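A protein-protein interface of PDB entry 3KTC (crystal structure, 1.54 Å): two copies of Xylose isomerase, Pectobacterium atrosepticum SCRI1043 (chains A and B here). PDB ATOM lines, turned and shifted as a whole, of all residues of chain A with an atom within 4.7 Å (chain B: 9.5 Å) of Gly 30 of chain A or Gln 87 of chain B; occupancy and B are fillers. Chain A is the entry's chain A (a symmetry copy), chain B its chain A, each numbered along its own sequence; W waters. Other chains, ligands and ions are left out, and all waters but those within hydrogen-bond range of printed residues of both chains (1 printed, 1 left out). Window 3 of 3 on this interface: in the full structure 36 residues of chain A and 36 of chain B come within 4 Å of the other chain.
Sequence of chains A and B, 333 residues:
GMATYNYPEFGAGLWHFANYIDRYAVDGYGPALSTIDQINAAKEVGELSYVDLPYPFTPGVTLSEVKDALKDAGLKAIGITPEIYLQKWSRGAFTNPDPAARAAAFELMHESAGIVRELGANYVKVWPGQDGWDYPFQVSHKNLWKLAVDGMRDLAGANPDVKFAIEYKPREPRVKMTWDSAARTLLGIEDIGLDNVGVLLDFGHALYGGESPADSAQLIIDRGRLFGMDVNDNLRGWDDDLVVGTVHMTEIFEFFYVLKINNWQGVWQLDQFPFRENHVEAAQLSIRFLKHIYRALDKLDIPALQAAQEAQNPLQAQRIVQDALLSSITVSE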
ATOM      1  N   ASN A  19      17.547   8.386  19.326  1.00  0.00           N
ATOM      2  CA  ASN A  19      18.706   8.187  20.183  1.00  0.00           C
ATOM      3  C   ASN A  19      19.073   9.545  20.739  1.00  0.00           C
ATOM      4  O   ASN A  19      18.846  10.571  20.105  1.00  0.00           O
ATOM      5  CB  ASN A  19      19.845   7.560  19.419  1.00  0.00           C
ATOM      6  CG  ASN A  19      19.592   6.094  19.137  1.00  0.00           C
ATOM      7  OD1 ASN A  19      19.015   5.388  19.981  1.00  0.00           O
ATOM      8  ND2 ASN A  19      20.012   5.628  17.974  1.00  0.00           N
ATOM      9  N   ALA A  25      28.046  12.215  27.207  1.00  0.00           N
ATOM     10  CA  ALA A  25      28.119  11.423  25.983  1.00  0.00           C
ATOM     11  C   ALA A  25      27.712  12.364  24.850  1.00  0.00           C
ATOM     12  O   ALA A  25      26.641  12.240  24.245  1.00  0.00           O
ATOM     13  CB  ALA A  25      27.183  10.159  26.048  1.00  0.00           C
ATOM     14  N   ASP A  27      28.838  12.552  21.991  1.00  0.00           N
ATOM     15  CA  ASP A  27      28.807  11.849  20.710  1.00  0.00           C
ATOM     16  C   ASP A  27      27.581  10.946  20.561  1.00  0.00           C
ATOM     17  O   ASP A  27      27.469  10.213  19.585  1.00  0.00           O
ATOM     18  CB  ASP A  27      30.123  11.095  20.425  1.00  0.00           C
ATOM     19  CG  ASP A  27      30.537  10.118  21.521  1.00  0.00           C
ATOM     20  OD1 ASP A  27      29.959  10.127  22.622  1.00  0.00           O
ATOM     21  OD2 ASP A  27      31.495   9.346  21.267  1.00  0.00           O
ATOM     22  N   GLY A  28      26.668  11.032  21.524  1.00  0.00           N
ATOM     23  CA  GLY A  28      25.346  10.421  21.420  1.00  0.00           C
ATOM     24  C   GLY A  28      25.268   9.023  21.961  1.00  0.00           C
ATOM     25  O   GLY A  28      26.270   8.375  22.089  1.00  0.00           O
ATOM     26  N   TYR A  29      24.052   8.608  22.302  1.00  0.00           N
ATOM     27  CA  TYR A  29      23.726   7.252  22.742  1.00  0.00           C
ATOM     28  C   TYR A  29      23.108   6.538  21.552  1.00  0.00           C
ATOM     29  O   TYR A  29      21.935   6.157  21.579  1.00  0.00           O
ATOM     30  CB  TYR A  29      22.704   7.253  23.886  1.00  0.00           C
ATOM     31  CG  TYR A  29      23.199   7.821  25.204  1.00  0.00           C
ATOM     32  CD1 TYR A  29      23.220   9.172  25.419  1.00  0.00           C
ATOM     33  CD2 TYR A  29      23.650   6.986  26.225  1.00  0.00           C
ATOM     34  CE1 TYR A  29      23.680   9.701  26.642  1.00  0.00           C
ATOM     35  CE2 TYR A  29      24.102   7.499  27.451  1.00  0.00           C
ATOM     36  CZ  TYR A  29      24.125   8.858  27.641  1.00  0.00           C
ATOM     37  OH  TYR A  29      24.570   9.378  28.843  1.00  0.00           O
ATOM     38  N   GLY A  30      23.846   6.492  20.468  1.00  0.00           N
ATOM     39  CA  GLY A  30      23.480   5.690  19.301  1.00  0.00           C
ATOM     40  C   GLY A  30      23.438   6.670  18.146  1.00  0.00           C
ATOM     41  O   GLY A  30      23.569   7.878  18.351  1.00  0.00           O
ATOM     42  N   PRO A  31      23.224   6.161  16.922  1.00  0.00           N
ATOM     43  CA  PRO A  31      23.202   7.013  15.732  1.00  0.00           C
ATOM     44  C   PRO A  31      21.948   7.895  15.622  1.00  0.00           C
ATOM     45  O   PRO A  31      20.892   7.576  16.183  1.00  0.00           O
ATOM     46  CB  PRO A  31      23.249   6.000  14.594  1.00  0.00           C
ATOM     47  CG  PRO A  31      22.599   4.790  15.146  1.00  0.00           C
ATOM     48  CD  PRO A  31      22.969   4.749  16.606  1.00  0.00           C
ATOM     49  N   ALA A  32      22.076   8.997  14.894  1.00  0.00           N
ATOM     50  CA  ALA A  32      20.970   9.917  14.694  1.00  0.00           C
ATOM     51  C   ALA A  32      19.930   9.233  13.824  1.00  0.00           C
ATOM     52  O   ALA A  32      20.253   8.688  12.778  1.00  0.00           O
ATOM     53  CB  ALA A  32      21.446  11.188  14.028  1.00  0.00           C
ATOM     54  N   GLU B  83      38.148  10.529  29.085  1.00  0.00           N
ATOM     55  CA  GLU B  83      36.729  10.641  28.740  1.00  0.00           C
ATOM     56  C   GLU B  83      36.061   9.269  28.592  1.00  0.00           C
ATOM     57  O   GLU B  83      35.713   8.833  27.498  1.00  0.00           O
ATOM     58  CB  GLU B  83      36.588  11.481  27.468  1.00  0.00           C
ATOM     59  CG  GLU B  83      37.076  12.900  27.690  1.00  0.00           C
ATOM     60  CD  GLU B  83      36.128  13.931  27.128  1.00  0.00           C
ATOM     61  OE1 GLU B  83      36.230  14.169  25.917  1.00  0.00           O
ATOM     62  OE2 GLU B  83      35.325  14.519  27.905  1.00  0.00           O
ATOM     63  N   ILE B  84      35.851   8.642  29.750  1.00  0.00           N
ATOM     64  CA  ILE B  84      35.353   7.283  29.866  1.00  0.00           C
ATOM     65  C   ILE B  84      33.830   7.221  29.961  1.00  0.00           C
ATOM     66  O   ILE B  84      33.276   6.236  30.403  1.00  0.00           O
ATOM     67  CB  ILE B  84      36.001   6.566  31.099  1.00  0.00           C
ATOM     68  CG1 ILE B  84      35.763   7.344  32.415  1.00  0.00           C
ATOM     69  CG2 ILE B  84      37.488   6.355  30.832  1.00  0.00           C
ATOM     70  CD1 ILE B  84      36.220   6.623  33.696  1.00  0.00           C
ATOM     71  N   TYR B  85      33.170   8.270  29.492  1.00  0.00           N
ATOM     72  CA  TYR B  85      31.721   8.425  29.575  1.00  0.00           C
ATOM     73  C   TYR B  85      31.096   8.757  28.212  1.00  0.00           C
ATOM     74  O   TYR B  85      29.902   9.082  28.139  1.00  0.00           O
ATOM     75  CB  TYR B  85      31.362   9.503  30.626  1.00  0.00           C
ATOM     76  CG  TYR B  85      32.335  10.664  30.591  1.00  0.00           C
ATOM     77  CD1 TYR B  85      32.252  11.635  29.595  1.00  0.00           C
ATOM     78  CD2 TYR B  85      33.401  10.733  31.483  1.00  0.00           C
ATOM     79  CE1 TYR B  85      33.147  12.660  29.526  1.00  0.00           C
ATOM     80  CE2 TYR B  85      34.310  11.766  31.408  1.00  0.00           C
ATOM     81  CZ  TYR B  85      34.173  12.729  30.427  1.00  0.00           C
ATOM     82  OH  TYR B  85      35.085  13.749  30.299  1.00  0.00           O
ATOM     83  N   LEU B  86      31.885   8.632  27.142  1.00  0.00           N
ATOM     84  CA  LEU B  86      31.444   8.840  25.773  1.00  0.00           C
ATOM     85  C   LEU B  86      30.650   7.622  25.318  1.00  0.00           C
ATOM     86  O   LEU B  86      30.548   6.619  26.039  1.00  0.00           O
ATOM     87  CB  LEU B  86      32.629   9.178  24.845  1.00  0.00           C
ATOM     88  CG  LEU B  86      33.389  10.460  25.237  1.00  0.00           C
ATOM     89  CD1 LEU B  86      34.652  10.709  24.366  1.00  0.00           C
ATOM     90  CD2 LEU B  86      32.495  11.678  25.152  1.00  0.00           C
ATOM     91  N   GLN B  87      30.087   7.716  24.115  1.00  0.00           N
ATOM     92  CA  GLN B  87      29.232   6.665  23.553  1.00  0.00           C
ATOM     93  C   GLN B  87      29.779   5.259  23.727  1.00  0.00           C
ATOM     94  O   GLN B  87      29.036   4.349  24.100  1.00  0.00           O
ATOM     95  CB  GLN B  87      28.992   6.889  22.059  1.00  0.00           C
ATOM     96  CG  GLN B  87      28.015   5.881  21.455  1.00  0.00           C
ATOM     97  CD  GLN B  87      27.743   6.108  19.977  1.00  0.00           C
ATOM     98  OE1 GLN B  87      28.110   5.277  19.145  1.00  0.00           O
ATOM     99  NE2 GLN B  87      27.103   7.230  19.639  1.00  0.00           N
ATOM    100  N   LYS B  88      31.068   5.079  23.459  1.00  0.00           N
ATOM    101  CA  LYS B  88      31.695   3.767  23.580  1.00  0.00           C
ATOM    102  C   LYS B  88      31.443   3.131  24.940  1.00  0.00           C
ATOM    103  O   LYS B  88      31.247   1.899  25.043  1.00  0.00           O
ATOM    104  CB  LYS B  88      33.206   3.889  23.344  1.00  0.00           C
ATOM    105  CG  LYS B  88      33.959   2.586  23.337  1.00  0.00           C
ATOM    106  CD  LYS B  88      35.362   2.850  22.820  1.00  0.00           C
ATOM    107  CE  LYS B  88      36.216   1.606  22.794  1.00  0.00           C
ATOM    108  NZ  LYS B  88      35.821   0.667  21.715  1.00  0.00           N
ATOM    109  N   TRP B  89      31.420   3.980  25.973  1.00  0.00           N
ATOM    110  CA  TRP B  89      31.225   3.536  27.336  1.00  0.00           C
ATOM    111  C   TRP B  89      29.901   4.015  27.904  1.00  0.00           C
ATOM    112  O   TRP B  89      29.727   4.160  29.125  1.00  0.00           O
ATOM    113  CB  TRP B  89      32.415   3.996  28.167  1.00  0.00           C
ATOM    114  CG  TRP B  89      33.697   3.357  27.684  1.00  0.00           C
ATOM    115  CD1 TRP B  89      34.007   2.046  27.749  1.00  0.00           C
ATOM    116  CD2 TRP B  89      34.796   4.009  27.056  1.00  0.00           C
ATOM    117  NE1 TRP B  89      35.232   1.823  27.190  1.00  0.00           N
ATOM    118  CE2 TRP B  89      35.743   3.016  26.757  1.00  0.00           C
ATOM    119  CE3 TRP B  89      35.062   5.334  26.683  1.00  0.00           C
ATOM    120  CZ2 TRP B  89      36.951   3.296  26.131  1.00  0.00           C
ATOM    121  CZ3 TRP B  89      36.261   5.612  26.082  1.00  0.00           C
ATOM    122  CH2 TRP B  89      37.195   4.606  25.813  1.00  0.00           C
ATOM    123  N   SER B  90      28.909   4.202  27.024  1.00  0.00           N
ATOM    124  CA  SER B  90      27.609   4.664  27.491  1.00  0.00           C
ATOM    125  C   SER B  90      26.907   3.698  28.443  1.00  0.00           C
ATOM    126  O   SER B  90      26.008   4.096  29.160  1.00  0.00           O
ATOM    127  CB  SER B  90      26.701   4.955  26.297  1.00  0.00           C
ATOM    128  OG  SER B  90      26.433   3.801  25.541  1.00  0.00           O
ATOM    129  N   ARG B  91      27.335   2.438  28.460  1.00  0.00           N
ATOM    130  CA  ARG B  91      26.802   1.440  29.393  1.00  0.00           C
ATOM    131  C   ARG B  91      27.823   1.059  30.462  1.00  0.00           C
ATOM    132  O   ARG B  91      27.628   0.097  31.199  1.00  0.00           O
ATOM    133  CB  ARG B  91      26.291   0.218  28.626  1.00  0.00           C
ATOM    134  CG  ARG B  91      25.199   0.586  27.616  1.00  0.00           C
ATOM    135  CD  ARG B  91      24.529  -0.608  27.024  1.00  0.00           C
ATOM    136  NE  ARG B  91      23.835  -1.301  28.086  1.00  0.00           N
ATOM    137  CZ  ARG B  91      23.794  -2.618  28.257  1.00  0.00           C
ATOM    138  NH1 ARG B  91      24.394  -3.442  27.418  1.00  0.00           N
ATOM    139  NH2 ARG B  91      23.162  -3.099  29.317  1.00  0.00           N
ATOM    140  N   GLY B  92      28.854   1.894  30.596  1.00  0.00           N
ATOM    141  CA  GLY B  92      29.875   1.748  31.635  1.00  0.00           C
ATOM    142  C   GLY B  92      31.287   1.711  31.081  1.00  0.00           C
ATOM    143  O   GLY B  92      31.517   1.353  29.915  1.00  0.00           O
ATOM    144  N   ALA B  93      32.228   2.093  31.945  1.00  0.00           N
ATOM    145  CA  ALA B  93      33.649   2.008  31.681  1.00  0.00           C
ATOM    146  C   ALA B  93      34.161   0.800  32.491  1.00  0.00           C
ATOM    147  O   ALA B  93      34.245  -0.312  31.963  1.00  0.00           O
ATOM    148  CB  ALA B  93      34.352   3.308  32.087  1.00  0.00           C
ATOM    149  N   ASN B  96      31.193  -1.736  32.459  1.00  0.00           N
ATOM    150  CA  ASN B  96      30.498  -2.166  31.242  1.00  0.00           C
ATOM    151  C   ASN B  96      30.221  -3.673  31.275  1.00  0.00           C
ATOM    152  O   ASN B  96      31.061  -4.432  31.707  1.00  0.00           O
ATOM    153  CB  ASN B  96      31.318  -1.841  29.993  1.00  0.00           C
ATOM    154  CG  ASN B  96      30.454  -1.714  28.758  1.00  0.00           C
ATOM    155  OD1 ASN B  96      29.988  -2.716  28.210  1.00  0.00           O
ATOM    156  ND2 ASN B  96      30.260  -0.480  28.289  1.00  0.00           N
ATOM    157  N   ALA B 101      34.818  -3.725  26.315  1.00  0.00           N
ATOM    158  CA  ALA B 101      34.636  -2.318  26.642  1.00  0.00           C
ATOM    159  C   ALA B 101      35.417  -1.945  27.907  1.00  0.00           C
ATOM    160  O   ALA B 101      36.005  -0.866  27.990  1.00  0.00           O
ATOM    161  CB  ALA B 101      33.159  -2.015  26.821  1.00  0.00           C
ATOM    162  N   GLN B 130      29.254   6.868  33.594  1.00  0.00           N
ATOM    163  CA  GLN B 130      28.310   5.905  33.043  1.00  0.00           C
ATOM    164  C   GLN B 130      28.256   4.617  33.854  1.00  0.00           C
ATOM    165  O   GLN B 130      27.583   3.671  33.450  1.00  0.00           O
ATOM    166  CB  GLN B 130      28.708   5.568  31.590  1.00  0.00           C
ATOM    167  CG  GLN B 130      28.717   6.781  30.625  1.00  0.00           C
ATOM    168  CD  GLN B 130      27.319   7.320  30.290  1.00  0.00           C
ATOM    169  OE1 GLN B 130      26.291   6.836  30.806  1.00  0.00           O
ATOM    170  NE2 GLN B 130      27.280   8.307  29.394  1.00  0.00           N
HETATM  171  O   HOH W   1      32.690   7.060  22.073  1.00  0.00           O
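No position is printed for both chains.
Water W1 lies within hydrogen-bond range of the side-chain carboxylate of Asp 27 of chain A (2.7 Å), the backbone NH of Lys 88 of chain B (2.9 Å) and the backbone NH of Gln 87 of chain B (3.4 Å).
The backbone carbonyl oxygen of Gln 87 of chain B is in hydrogen-bond range of the side-chain hydroxyl of Ser 90 of chain B (3.0 Å). OE2 of Glu 83 of chain B sits at hydrogen-bond distance from OH of Tyr 85 of chain B (2.5 Å). The backbone carbonyl oxygen (O) of Ser 90 of chain B sits close to the side-chain amide oxygen (OE1) of Gln 130 of chain B (3.2 Å). The side-chain amide nitrogen (NE2) of Gln 130 of chain B lies within hydrogen-bond range of the backbone carbonyl oxygen (O) of Tyr 85 of chain B (3.0 Å). The side-chain amide oxygen (OD1) of Asn 19 of chain A sits close to the backbone carbonyl oxygen (O) of Tyr 29 of chain A, 3.4 Å away.
Of the 8 printed residues of chain A, 5 touch a printed residue of chain B. Printed residues of chain B that touch a printed residue of chain A: Tyr 85, Leu 86, Gln 87, Ser 90 and Gln 130. Among the printed residues, 8 pairs touch across the chains.
Printed residues of chain B within 4 Å of Ala 25 of chain A: Tyr 85 and Gln 130. Printed residues of chain B within 4 Å of Asp 27 of chain A: Leu 86 and Gln 87. Of the printed residues of chain B, Tyr 29 of chain A touches Ser 90 (3.7 Å) and Gln 130 (3.0 Å). Printed residues of chain B within 4 Å of Gly 30 of chain A: Gln 87 (3.4 Å). Glu 83 of chain B touches none of the printed residues of chain A. Printed residues of chain A within 4 Å of Tyr 85 of chain B: Ala 25. Of the printed residues of chain A, Gln 87 of chain B touches Asp 27, Gly 28 and Gly 30. Trp 89 of chain B touches none of the printed residues of chain A. The nearest printed residue of chain B that does not touch Gly 30 of chain A is Ser 90 of chain B (6.3 Å). The nearest printed residue of chain B that does not touch Asp 27 of chain A is Lys 88 of chain B (4.8 Å).
The side-chain amide nitrogen (NE2) of Gln 130 of chain B is in hydrogen-bond range of the side-chain hydroxyl (OH) of Tyr 29 of chain A (3.0 Å). The side-chain amide nitrogen (NE2) of Gln 87 of chain B sits close to the backbone NH (N) of Gly 30 of chain A (3.4 Å). The backbone NH of Gln 87 of chain B sits at hydrogen-bond distance from the side-chain carboxylate of Asp 27 of chain A. NE2 of Gln 87 of chain B sits at hydrogen-bond distance from O of Gly 28 of chain A, at 2.8 Å.
Among the printed residues, pairs that only touch across the chains: Ala 25 of chain A with Tyr 85 of chain B (3.6 Å), Asp 27 of chain A with Leu 86 of chain B (3.6 Å), Tyr 29 of chain A with Ser 90 of chain B (3.7 Å) and Ala 25 of chain A with Gln 130 of chain B (3.8 Å).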
